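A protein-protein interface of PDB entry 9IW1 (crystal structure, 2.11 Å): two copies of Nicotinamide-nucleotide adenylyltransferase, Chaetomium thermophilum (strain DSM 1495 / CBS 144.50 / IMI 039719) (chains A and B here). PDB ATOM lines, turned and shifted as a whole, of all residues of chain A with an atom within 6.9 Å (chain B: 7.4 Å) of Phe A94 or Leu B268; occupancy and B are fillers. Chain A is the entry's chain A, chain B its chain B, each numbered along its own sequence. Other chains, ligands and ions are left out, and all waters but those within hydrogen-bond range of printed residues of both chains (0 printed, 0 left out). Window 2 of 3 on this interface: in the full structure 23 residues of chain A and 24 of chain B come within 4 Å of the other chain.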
ATOM      1  N   LYS A  63       1.157 -23.034 -10.091  1.00  0.00           N
ATOM      2  CA  LYS A  63       2.257 -22.632  -9.228  1.00  0.00           C
ATOM      3  C   LYS A  63       1.988 -21.240  -8.672  1.00  0.00           C
ATOM      4  O   LYS A  63       1.527 -20.350  -9.389  1.00  0.00           O
ATOM      5  CB  LYS A  63       3.587 -22.644  -9.996  1.00  0.00           C
ATOM      6  CG  LYS A  63       4.594 -23.695  -9.524  1.00  0.00           C
ATOM      7  CD  LYS A  63       4.079 -25.114  -9.702  1.00  0.00           C
ATOM      8  CE  LYS A  63       5.090 -26.156  -9.199  1.00  0.00           C
ATOM      9  NZ  LYS A  63       6.088 -26.555 -10.229  1.00  0.00           N
ATOM     10  N   ARG A  83      25.256 -17.876  -4.236  1.00  0.00           N
ATOM     11  CA  ARG A  83      24.919 -19.290  -4.365  1.00  0.00           C
ATOM     12  C   ARG A  83      23.637 -19.642  -3.616  1.00  0.00           C
ATOM     13  O   ARG A  83      22.883 -20.512  -4.061  1.00  0.00           O
ATOM     14  CB  ARG A  83      26.101 -20.140  -3.888  1.00  0.00           C
ATOM     15  CG  ARG A  83      25.919 -21.641  -4.049  1.00  0.00           C
ATOM     16  CD  ARG A  83      25.670 -22.017  -5.486  1.00  0.00           C
ATOM     17  NE  ARG A  83      25.214 -23.398  -5.589  1.00  0.00           N
ATOM     18  CZ  ARG A  83      24.689 -23.930  -6.685  1.00  0.00           C
ATOM     19  NH1 ARG A  83      24.619 -23.250  -7.821  1.00  0.00           N
ATOM     20  NH2 ARG A  83      24.211 -25.170  -6.637  1.00  0.00           N
ATOM     21  N   SER A  89      16.454 -21.502  -5.566  1.00  0.00           N
ATOM     22  CA  SER A  89      15.768 -21.727  -6.837  1.00  0.00           C
ATOM     23  C   SER A  89      15.607 -23.219  -7.123  1.00  0.00           C
ATOM     24  O   SER A  89      14.506 -23.686  -7.435  1.00  0.00           O
ATOM     25  CB  SER A  89      16.543 -21.035  -7.958  1.00  0.00           C
ATOM     26  OG  SER A  89      15.862 -21.095  -9.196  1.00  0.00           O
ATOM     27  N   ASP A  90      16.694 -23.985  -6.989  1.00  0.00           N
ATOM     28  CA  ASP A  90      16.655 -25.430  -7.221  1.00  0.00           C
ATOM     29  C   ASP A  90      15.713 -26.145  -6.253  1.00  0.00           C
ATOM     30  O   ASP A  90      15.004 -27.078  -6.644  1.00  0.00           O
ATOM     31  CB  ASP A  90      18.065 -26.010  -7.101  1.00  0.00           C
ATOM     32  CG  ASP A  90      18.926 -25.711  -8.314  1.00  0.00           C
ATOM     33  OD1 ASP A  90      18.385 -25.226  -9.330  1.00  0.00           O
ATOM     34  OD2 ASP A  90      20.149 -25.951  -8.245  1.00  0.00           O
ATOM     35  N   PHE A  91      15.749 -25.774  -4.972  1.00  0.00           N
ATOM     36  CA  PHE A  91      14.871 -26.402  -3.990  1.00  0.00           C
ATOM     37  C   PHE A  91      13.409 -26.138  -4.321  1.00  0.00           C
ATOM     38  O   PHE A  91      12.573 -27.044  -4.231  1.00  0.00           O
ATOM     39  CB  PHE A  91      15.207 -25.891  -2.588  1.00  0.00           C
ATOM     40  CG  PHE A  91      14.246 -26.345  -1.517  1.00  0.00           C
ATOM     41  CD1 PHE A  91      14.452 -27.533  -0.844  1.00  0.00           C
ATOM     42  CD2 PHE A  91      13.156 -25.566  -1.161  1.00  0.00           C
ATOM     43  CE1 PHE A  91      13.581 -27.947   0.148  1.00  0.00           C
ATOM     44  CE2 PHE A  91      12.279 -25.975  -0.164  1.00  0.00           C
ATOM     45  CZ  PHE A  91      12.494 -27.164   0.492  1.00  0.00           C
ATOM     46  N   VAL A  92      13.084 -24.893  -4.694  1.00  0.00           N
ATOM     47  CA  VAL A  92      11.707 -24.530  -5.005  1.00  0.00           C
ATOM     48  C   VAL A  92      11.187 -25.353  -6.172  1.00  0.00           C
ATOM     49  O   VAL A  92      10.049 -25.837  -6.152  1.00  0.00           O
ATOM     50  CB  VAL A  92      11.606 -23.022  -5.285  1.00  0.00           C
ATOM     51  CG1 VAL A  92      10.408 -22.720  -6.179  1.00  0.00           C
ATOM     52  CG2 VAL A  92      11.503 -22.256  -3.972  1.00  0.00           C
ATOM     53  N   ARG A  93      12.020 -25.530  -7.202  1.00  0.00           N
ATOM     54  CA  ARG A  93      11.593 -26.256  -8.393  1.00  0.00           C
ATOM     55  C   ARG A  93      11.169 -27.682  -8.054  1.00  0.00           C
ATOM     56  O   ARG A  93      10.167 -28.178  -8.578  1.00  0.00           O
ATOM     57  CB  ARG A  93      12.719 -26.266  -9.434  1.00  0.00           C
ATOM     58  CG  ARG A  93      12.995 -24.918 -10.110  1.00  0.00           C
ATOM     59  CD  ARG A  93      14.337 -24.936 -10.863  1.00  0.00           C
ATOM     60  NE  ARG A  93      14.376 -25.975 -11.888  1.00  0.00           N
ATOM     61  CZ  ARG A  93      15.477 -26.589 -12.304  1.00  0.00           C
ATOM     62  NH1 ARG A  93      16.660 -26.330 -11.771  1.00  0.00           N
ATOM     63  NH2 ARG A  93      15.384 -27.501 -13.267  1.00  0.00           N
ATOM     64  N   PHE A  94      11.901 -28.348  -7.165  1.00  0.00           N
ATOM     65  CA  PHE A  94      11.728 -29.780  -6.964  1.00  0.00           C
ATOM     66  C   PHE A  94      11.051 -30.140  -5.652  1.00  0.00           C
ATOM     67  O   PHE A  94      10.790 -31.324  -5.420  1.00  0.00           O
ATOM     68  CB  PHE A  94      13.091 -30.489  -7.066  1.00  0.00           C
ATOM     69  CG  PHE A  94      13.708 -30.408  -8.444  1.00  0.00           C
ATOM     70  CD1 PHE A  94      13.232 -31.205  -9.477  1.00  0.00           C
ATOM     71  CD2 PHE A  94      14.734 -29.517  -8.713  1.00  0.00           C
ATOM     72  CE1 PHE A  94      13.778 -31.125 -10.749  1.00  0.00           C
ATOM     73  CE2 PHE A  94      15.282 -29.429  -9.986  1.00  0.00           C
ATOM     74  CZ  PHE A  94      14.802 -30.238 -11.004  1.00  0.00           C
ATOM     75  N   ASN A  95      10.750 -29.165  -4.791  1.00  0.00           N
ATOM     76  CA  ASN A  95      10.185 -29.468  -3.487  1.00  0.00           C
ATOM     77  C   ASN A  95       8.986 -28.612  -3.103  1.00  0.00           C
ATOM     78  O   ASN A  95       8.466 -28.784  -1.998  1.00  0.00           O
ATOM     79  CB  ASN A  95      11.255 -29.340  -2.397  1.00  0.00           C
ATOM     80  CG  ASN A  95      12.410 -30.294  -2.609  1.00  0.00           C
ATOM     81  OD1 ASN A  95      13.317 -30.029  -3.403  1.00  0.00           O
ATOM     82  ND2 ASN A  95      12.374 -31.424  -1.915  1.00  0.00           N
ATOM     83  N   THR A  96       8.561 -27.672  -3.940  1.00  0.00           N
ATOM     84  CA  THR A  96       7.455 -26.789  -3.597  1.00  0.00           C
ATOM     85  C   THR A  96       6.527 -26.650  -4.790  1.00  0.00           C
ATOM     86  O   THR A  96       6.818 -27.116  -5.895  1.00  0.00           O
ATOM     87  CB  THR A  96       7.920 -25.380  -3.192  1.00  0.00           C
ATOM     88  OG1 THR A  96       8.349 -24.657  -4.361  1.00  0.00           O
ATOM     89  CG2 THR A  96       9.042 -25.443  -2.188  1.00  0.00           C
ATOM     90  N   LYS B 259      30.999 -33.275  -8.118  1.00  0.00           N
ATOM     91  CA  LYS B 259      29.716 -32.733  -7.694  1.00  0.00           C
ATOM     92  C   LYS B 259      29.134 -31.814  -8.755  1.00  0.00           C
ATOM     93  O   LYS B 259      27.922 -31.837  -8.998  1.00  0.00           O
ATOM     94  CB  LYS B 259      29.861 -32.012  -6.359  1.00  0.00           C
ATOM     95  CG  LYS B 259      30.246 -32.943  -5.238  1.00  0.00           C
ATOM     96  CD  LYS B 259      31.206 -32.269  -4.277  1.00  0.00           C
ATOM     97  CE  LYS B 259      31.001 -32.738  -2.845  1.00  0.00           C
ATOM     98  NZ  LYS B 259      31.724 -34.015  -2.574  1.00  0.00           N
ATOM     99  N   VAL B 260      29.978 -31.036  -9.435  1.00  0.00           N
ATOM    100  CA  VAL B 260      29.456 -30.141 -10.465  1.00  0.00           C
ATOM    101  C   VAL B 260      28.822 -30.945 -11.598  1.00  0.00           C
ATOM    102  O   VAL B 260      27.762 -30.575 -12.116  1.00  0.00           O
ATOM    103  CB  VAL B 260      30.555 -29.185 -10.970  1.00  0.00           C
ATOM    104  CG1 VAL B 260      30.085 -28.439 -12.213  1.00  0.00           C
ATOM    105  CG2 VAL B 260      30.941 -28.190  -9.867  1.00  0.00           C
ATOM    106  N   LEU B 262      27.473 -33.988 -11.343  1.00  0.00           N
ATOM    107  CA  LEU B 262      26.224 -34.522 -10.807  1.00  0.00           C
ATOM    108  C   LEU B 262      25.104 -33.488 -10.880  1.00  0.00           C
ATOM    109  O   LEU B 262      24.013 -33.771 -11.390  1.00  0.00           O
ATOM    110  CB  LEU B 262      26.435 -34.993  -9.371  1.00  0.00           C
ATOM    111  CG  LEU B 262      25.199 -35.553  -8.667  1.00  0.00           C
ATOM    112  CD1 LEU B 262      24.654 -36.752  -9.431  1.00  0.00           C
ATOM    113  CD2 LEU B 262      25.531 -35.936  -7.234  1.00  0.00           C
ATOM    114  N   PHE B 263      25.366 -32.273 -10.390  1.00  0.00           N
ATOM    115  CA  PHE B 263      24.367 -31.213 -10.475  1.00  0.00           C
ATOM    116  C   PHE B 263      23.935 -30.978 -11.914  1.00  0.00           C
ATOM    117  O   PHE B 263      22.743 -30.788 -12.190  1.00  0.00           O
ATOM    118  CB  PHE B 263      24.925 -29.922  -9.872  1.00  0.00           C
ATOM    119  CG  PHE B 263      24.784 -29.837  -8.378  1.00  0.00           C
ATOM    120  CD1 PHE B 263      24.999 -30.952  -7.582  1.00  0.00           C
ATOM    121  CD2 PHE B 263      24.449 -28.638  -7.769  1.00  0.00           C
ATOM    122  CE1 PHE B 263      24.876 -30.879  -6.210  1.00  0.00           C
ATOM    123  CE2 PHE B 263      24.328 -28.557  -6.392  1.00  0.00           C
ATOM    124  CZ  PHE B 263      24.547 -29.677  -5.614  1.00  0.00           C
ATOM    125  N   LEU B 264      24.888 -30.984 -12.845  1.00  0.00           N
ATOM    126  CA  LEU B 264      24.558 -30.775 -14.253  1.00  0.00           C
ATOM    127  C   LEU B 264      23.682 -31.898 -14.801  1.00  0.00           C
ATOM    128  O   LEU B 264      22.767 -31.642 -15.593  1.00  0.00           O
ATOM    129  CB  LEU B 264      25.835 -30.649 -15.081  1.00  0.00           C
ATOM    130  CG  LEU B 264      26.626 -29.353 -14.892  1.00  0.00           C
ATOM    131  CD1 LEU B 264      28.009 -29.470 -15.521  1.00  0.00           C
ATOM    132  CD2 LEU B 264      25.868 -28.172 -15.471  1.00  0.00           C
ATOM    133  N   ARG B 265      23.946 -33.141 -14.393  1.00  0.00           N
ATOM    134  CA  ARG B 265      23.137 -34.260 -14.867  1.00  0.00           C
ATOM    135  C   ARG B 265      21.717 -34.177 -14.333  1.00  0.00           C
ATOM    136  O   ARG B 265      20.760 -34.482 -15.052  1.00  0.00           O
ATOM    137  CB  ARG B 265      23.771 -35.593 -14.459  1.00  0.00           C
ATOM    138  CG  ARG B 265      24.849 -36.101 -15.390  1.00  0.00           C
ATOM    139  CD  ARG B 265      25.052 -37.606 -15.212  1.00  0.00           C
ATOM    140  NE  ARG B 265      25.456 -37.948 -13.852  1.00  0.00           N
ATOM    141  CZ  ARG B 265      26.637 -37.650 -13.321  1.00  0.00           C
ATOM    142  NH1 ARG B 265      27.552 -36.981 -14.005  1.00  0.00           N
ATOM    143  NH2 ARG B 265      26.902 -38.024 -12.070  1.00  0.00           N
ATOM    144  N   LYS B 266      21.559 -33.751 -13.085  1.00  0.00           N
ATOM    145  CA  LYS B 266      20.251 -33.650 -12.456  1.00  0.00           C
ATOM    146  C   LYS B 266      19.559 -32.328 -12.758  1.00  0.00           C
ATOM    147  O   LYS B 266      18.547 -32.020 -12.121  1.00  0.00           O
ATOM    148  CB  LYS B 266      20.384 -33.874 -10.947  1.00  0.00           C
ATOM    149  CG  LYS B 266      21.174 -35.146 -10.609  1.00  0.00           C
ATOM    150  CD  LYS B 266      20.789 -35.730  -9.255  1.00  0.00           C
ATOM    151  CE  LYS B 266      21.103 -34.774  -8.121  1.00  0.00           C
ATOM    152  NZ  LYS B 266      20.780 -35.330  -6.771  1.00  0.00           N
ATOM    153  N   ASP B 267      20.082 -31.556 -13.721  1.00  0.00           N
ATOM    154  CA  ASP B 267      19.479 -30.290 -14.154  1.00  0.00           C
ATOM    155  C   ASP B 267      19.400 -29.271 -13.018  1.00  0.00           C
ATOM    156  O   ASP B 267      18.471 -28.466 -12.951  1.00  0.00           O
ATOM    157  CB  ASP B 267      18.094 -30.525 -14.759  1.00  0.00           C
ATOM    158  CG  ASP B 267      17.708 -29.460 -15.755  1.00  0.00           C
ATOM    159  OD1 ASP B 267      18.591 -29.023 -16.516  1.00  0.00           O
ATOM    160  OD2 ASP B 267      16.520 -29.071 -15.786  1.00  0.00           O
ATOM    161  N   LEU B 268      20.402 -29.272 -12.146  1.00  0.00           N
ATOM    162  CA  LEU B 268      20.524 -28.269 -11.100  1.00  0.00           C
ATOM    163  C   LEU B 268      21.490 -27.163 -11.526  1.00  0.00           C
ATOM    164  O   LEU B 268      22.316 -27.331 -12.428  1.00  0.00           O
ATOM    165  CB  LEU B 268      20.987 -28.915  -9.790  1.00  0.00           C
ATOM    166  CG  LEU B 268      20.116 -30.084  -9.296  1.00  0.00           C
ATOM    167  CD1 LEU B 268      20.768 -30.823  -8.144  1.00  0.00           C
ATOM    168  CD2 LEU B 268      18.745 -29.588  -8.886  1.00  0.00           C
ATOM    169  N   SER B 269      21.361 -26.010 -10.884  1.00  0.00           N
ATOM    170  CA  SER B 269      22.203 -24.868 -11.207  1.00  0.00           C
ATOM    171  C   SER B 269      23.609 -25.073 -10.663  1.00  0.00           C
ATOM    172  O   SER B 269      23.792 -25.612  -9.571  1.00  0.00           O
ATOM    173  CB  SER B 269      21.621 -23.587 -10.617  1.00  0.00           C
ATOM    174  OG  SER B 269      22.487 -22.493 -10.868  1.00  0.00           O
ATOM    175  N   VAL B 270      24.612 -24.654 -11.437  1.00  0.00           N
ATOM    176  CA  VAL B 270      25.982 -24.609 -10.940  1.00  0.00           C
ATOM    177  C   VAL B 270      26.534 -23.190 -10.936  1.00  0.00           C
ATOM    178  O   VAL B 270      27.732 -22.996 -10.727  1.00  0.00           O
ATOM    179  CB  VAL B 270      26.920 -25.552 -11.724  1.00  0.00           C
ATOM    180  CG1 VAL B 270      26.562 -27.021 -11.483  1.00  0.00           C
ATOM    181  CG2 VAL B 270      26.902 -25.205 -13.201  1.00  0.00           C
ATOM    182  N   ARG B 271      25.687 -22.190 -11.166  1.00  0.00           N
ATOM    183  CA  ARG B 271      26.163 -20.816 -11.114  1.00  0.00           C
ATOM    184  C   ARG B 271      26.694 -20.513  -9.714  1.00  0.00           C
ATOM    185  O   ARG B 271      26.111 -20.929  -8.709  1.00  0.00           O
ATOM    186  CB  ARG B 271      25.043 -19.845 -11.502  1.00  0.00           C
ATOM    187  CG  ARG B 271      25.583 -18.522 -12.028  1.00  0.00           C
ATOM    188  CD  ARG B 271      24.509 -17.507 -12.384  1.00  0.00           C
ATOM    189  NE  ARG B 271      23.783 -17.843 -13.604  1.00  0.00           N
ATOM    190  CZ  ARG B 271      24.306 -17.882 -14.824  1.00  0.00           C
ATOM    191  NH1 ARG B 271      25.598 -17.676 -15.035  1.00  0.00           N
ATOM    192  NH2 ARG B 271      23.515 -18.158 -15.860  1.00  0.00           N
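Of the 12 printed residues of chain B, 6 touch a printed residue of chain A. Hydrophobic or aromatic side chains of chain B that line the printed part of chain A: Phe B263 and Leu B268. Among the printed residues, 8 pairs touch across the chains. Among the printed residues, Asp or Glu carboxylates within 4 Å of a Lys or Arg side-chain nitrogen of the other chain: Arg A93 with Asp B267 (3.2 Å).
The side-chain carboxylate (OD2) of Asp B267 is in salt-bridge range of the guanidinium group (NH2) of Arg A93 (3.2 Å). O of Arg B271 sits at hydrogen-bond distance from NH1 of Arg A83 (2.9 Å). The side-chain carboxylate (OD2) of Asp A90 sits at hydrogen-bond distance from the backbone NH (N) of Ser B269 (2.9 Å). The backbone carbonyl oxygen (O) of Ser B269 lies within hydrogen-bond range of the guanidinium group (NH2) of Arg A83.
Among the printed residues, merely in contact across the chains: Arg A83 with Phe B263, Asp A90 with Leu B268, Phe A94 with Leu B268 and Arg A83 with Val B270.
Of the printed residues of chain B, Arg A83 touches Phe B263, Ser B269, Val B270 and Arg B271. Of the printed residues of chain B, Asp A90 touches Leu B268 (3.4 Å) and Ser B269 (2.9 Å). Phe A91 touches none of the printed residues of chain B. Phe A94 touches one residue of chain B. Asn A95 touches none of the printed residues of chain B. Of the printed residues of chain A, Phe B263 touches Arg A83. Printed residues of chain A within 4 Å of Asp B267: Arg A93. Leu B268 touches just these residues of chain A: Asp A90 (3.4 Å) and Phe A94 (3.6 Å). Printed residues of chain A within 4 Å of Ser B269: Arg A83 (3.0 Å) and Asp A90 (2.9 Å). The nearest residue of chain A that does not touch Leu B268 is Arg A93 (4.4 Å). The nearest printed residue of chain B that does not touch Arg A83 is Leu B268 (5.9 Å).
No position is printed for both chains.
The backbone carbonyl oxygen of Phe B263 lies within hydrogen-bond range of the backbone NH of Leu B268, at 2.8 Å. N of Arg B271 lies within hydrogen-bond range of OG of Ser B269 (3.2 Å). The guanidinium group (NH1) of Arg A93 is in salt-bridge range of the side-chain carboxylate (OD1) of Asp A90 (3.2 Å).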
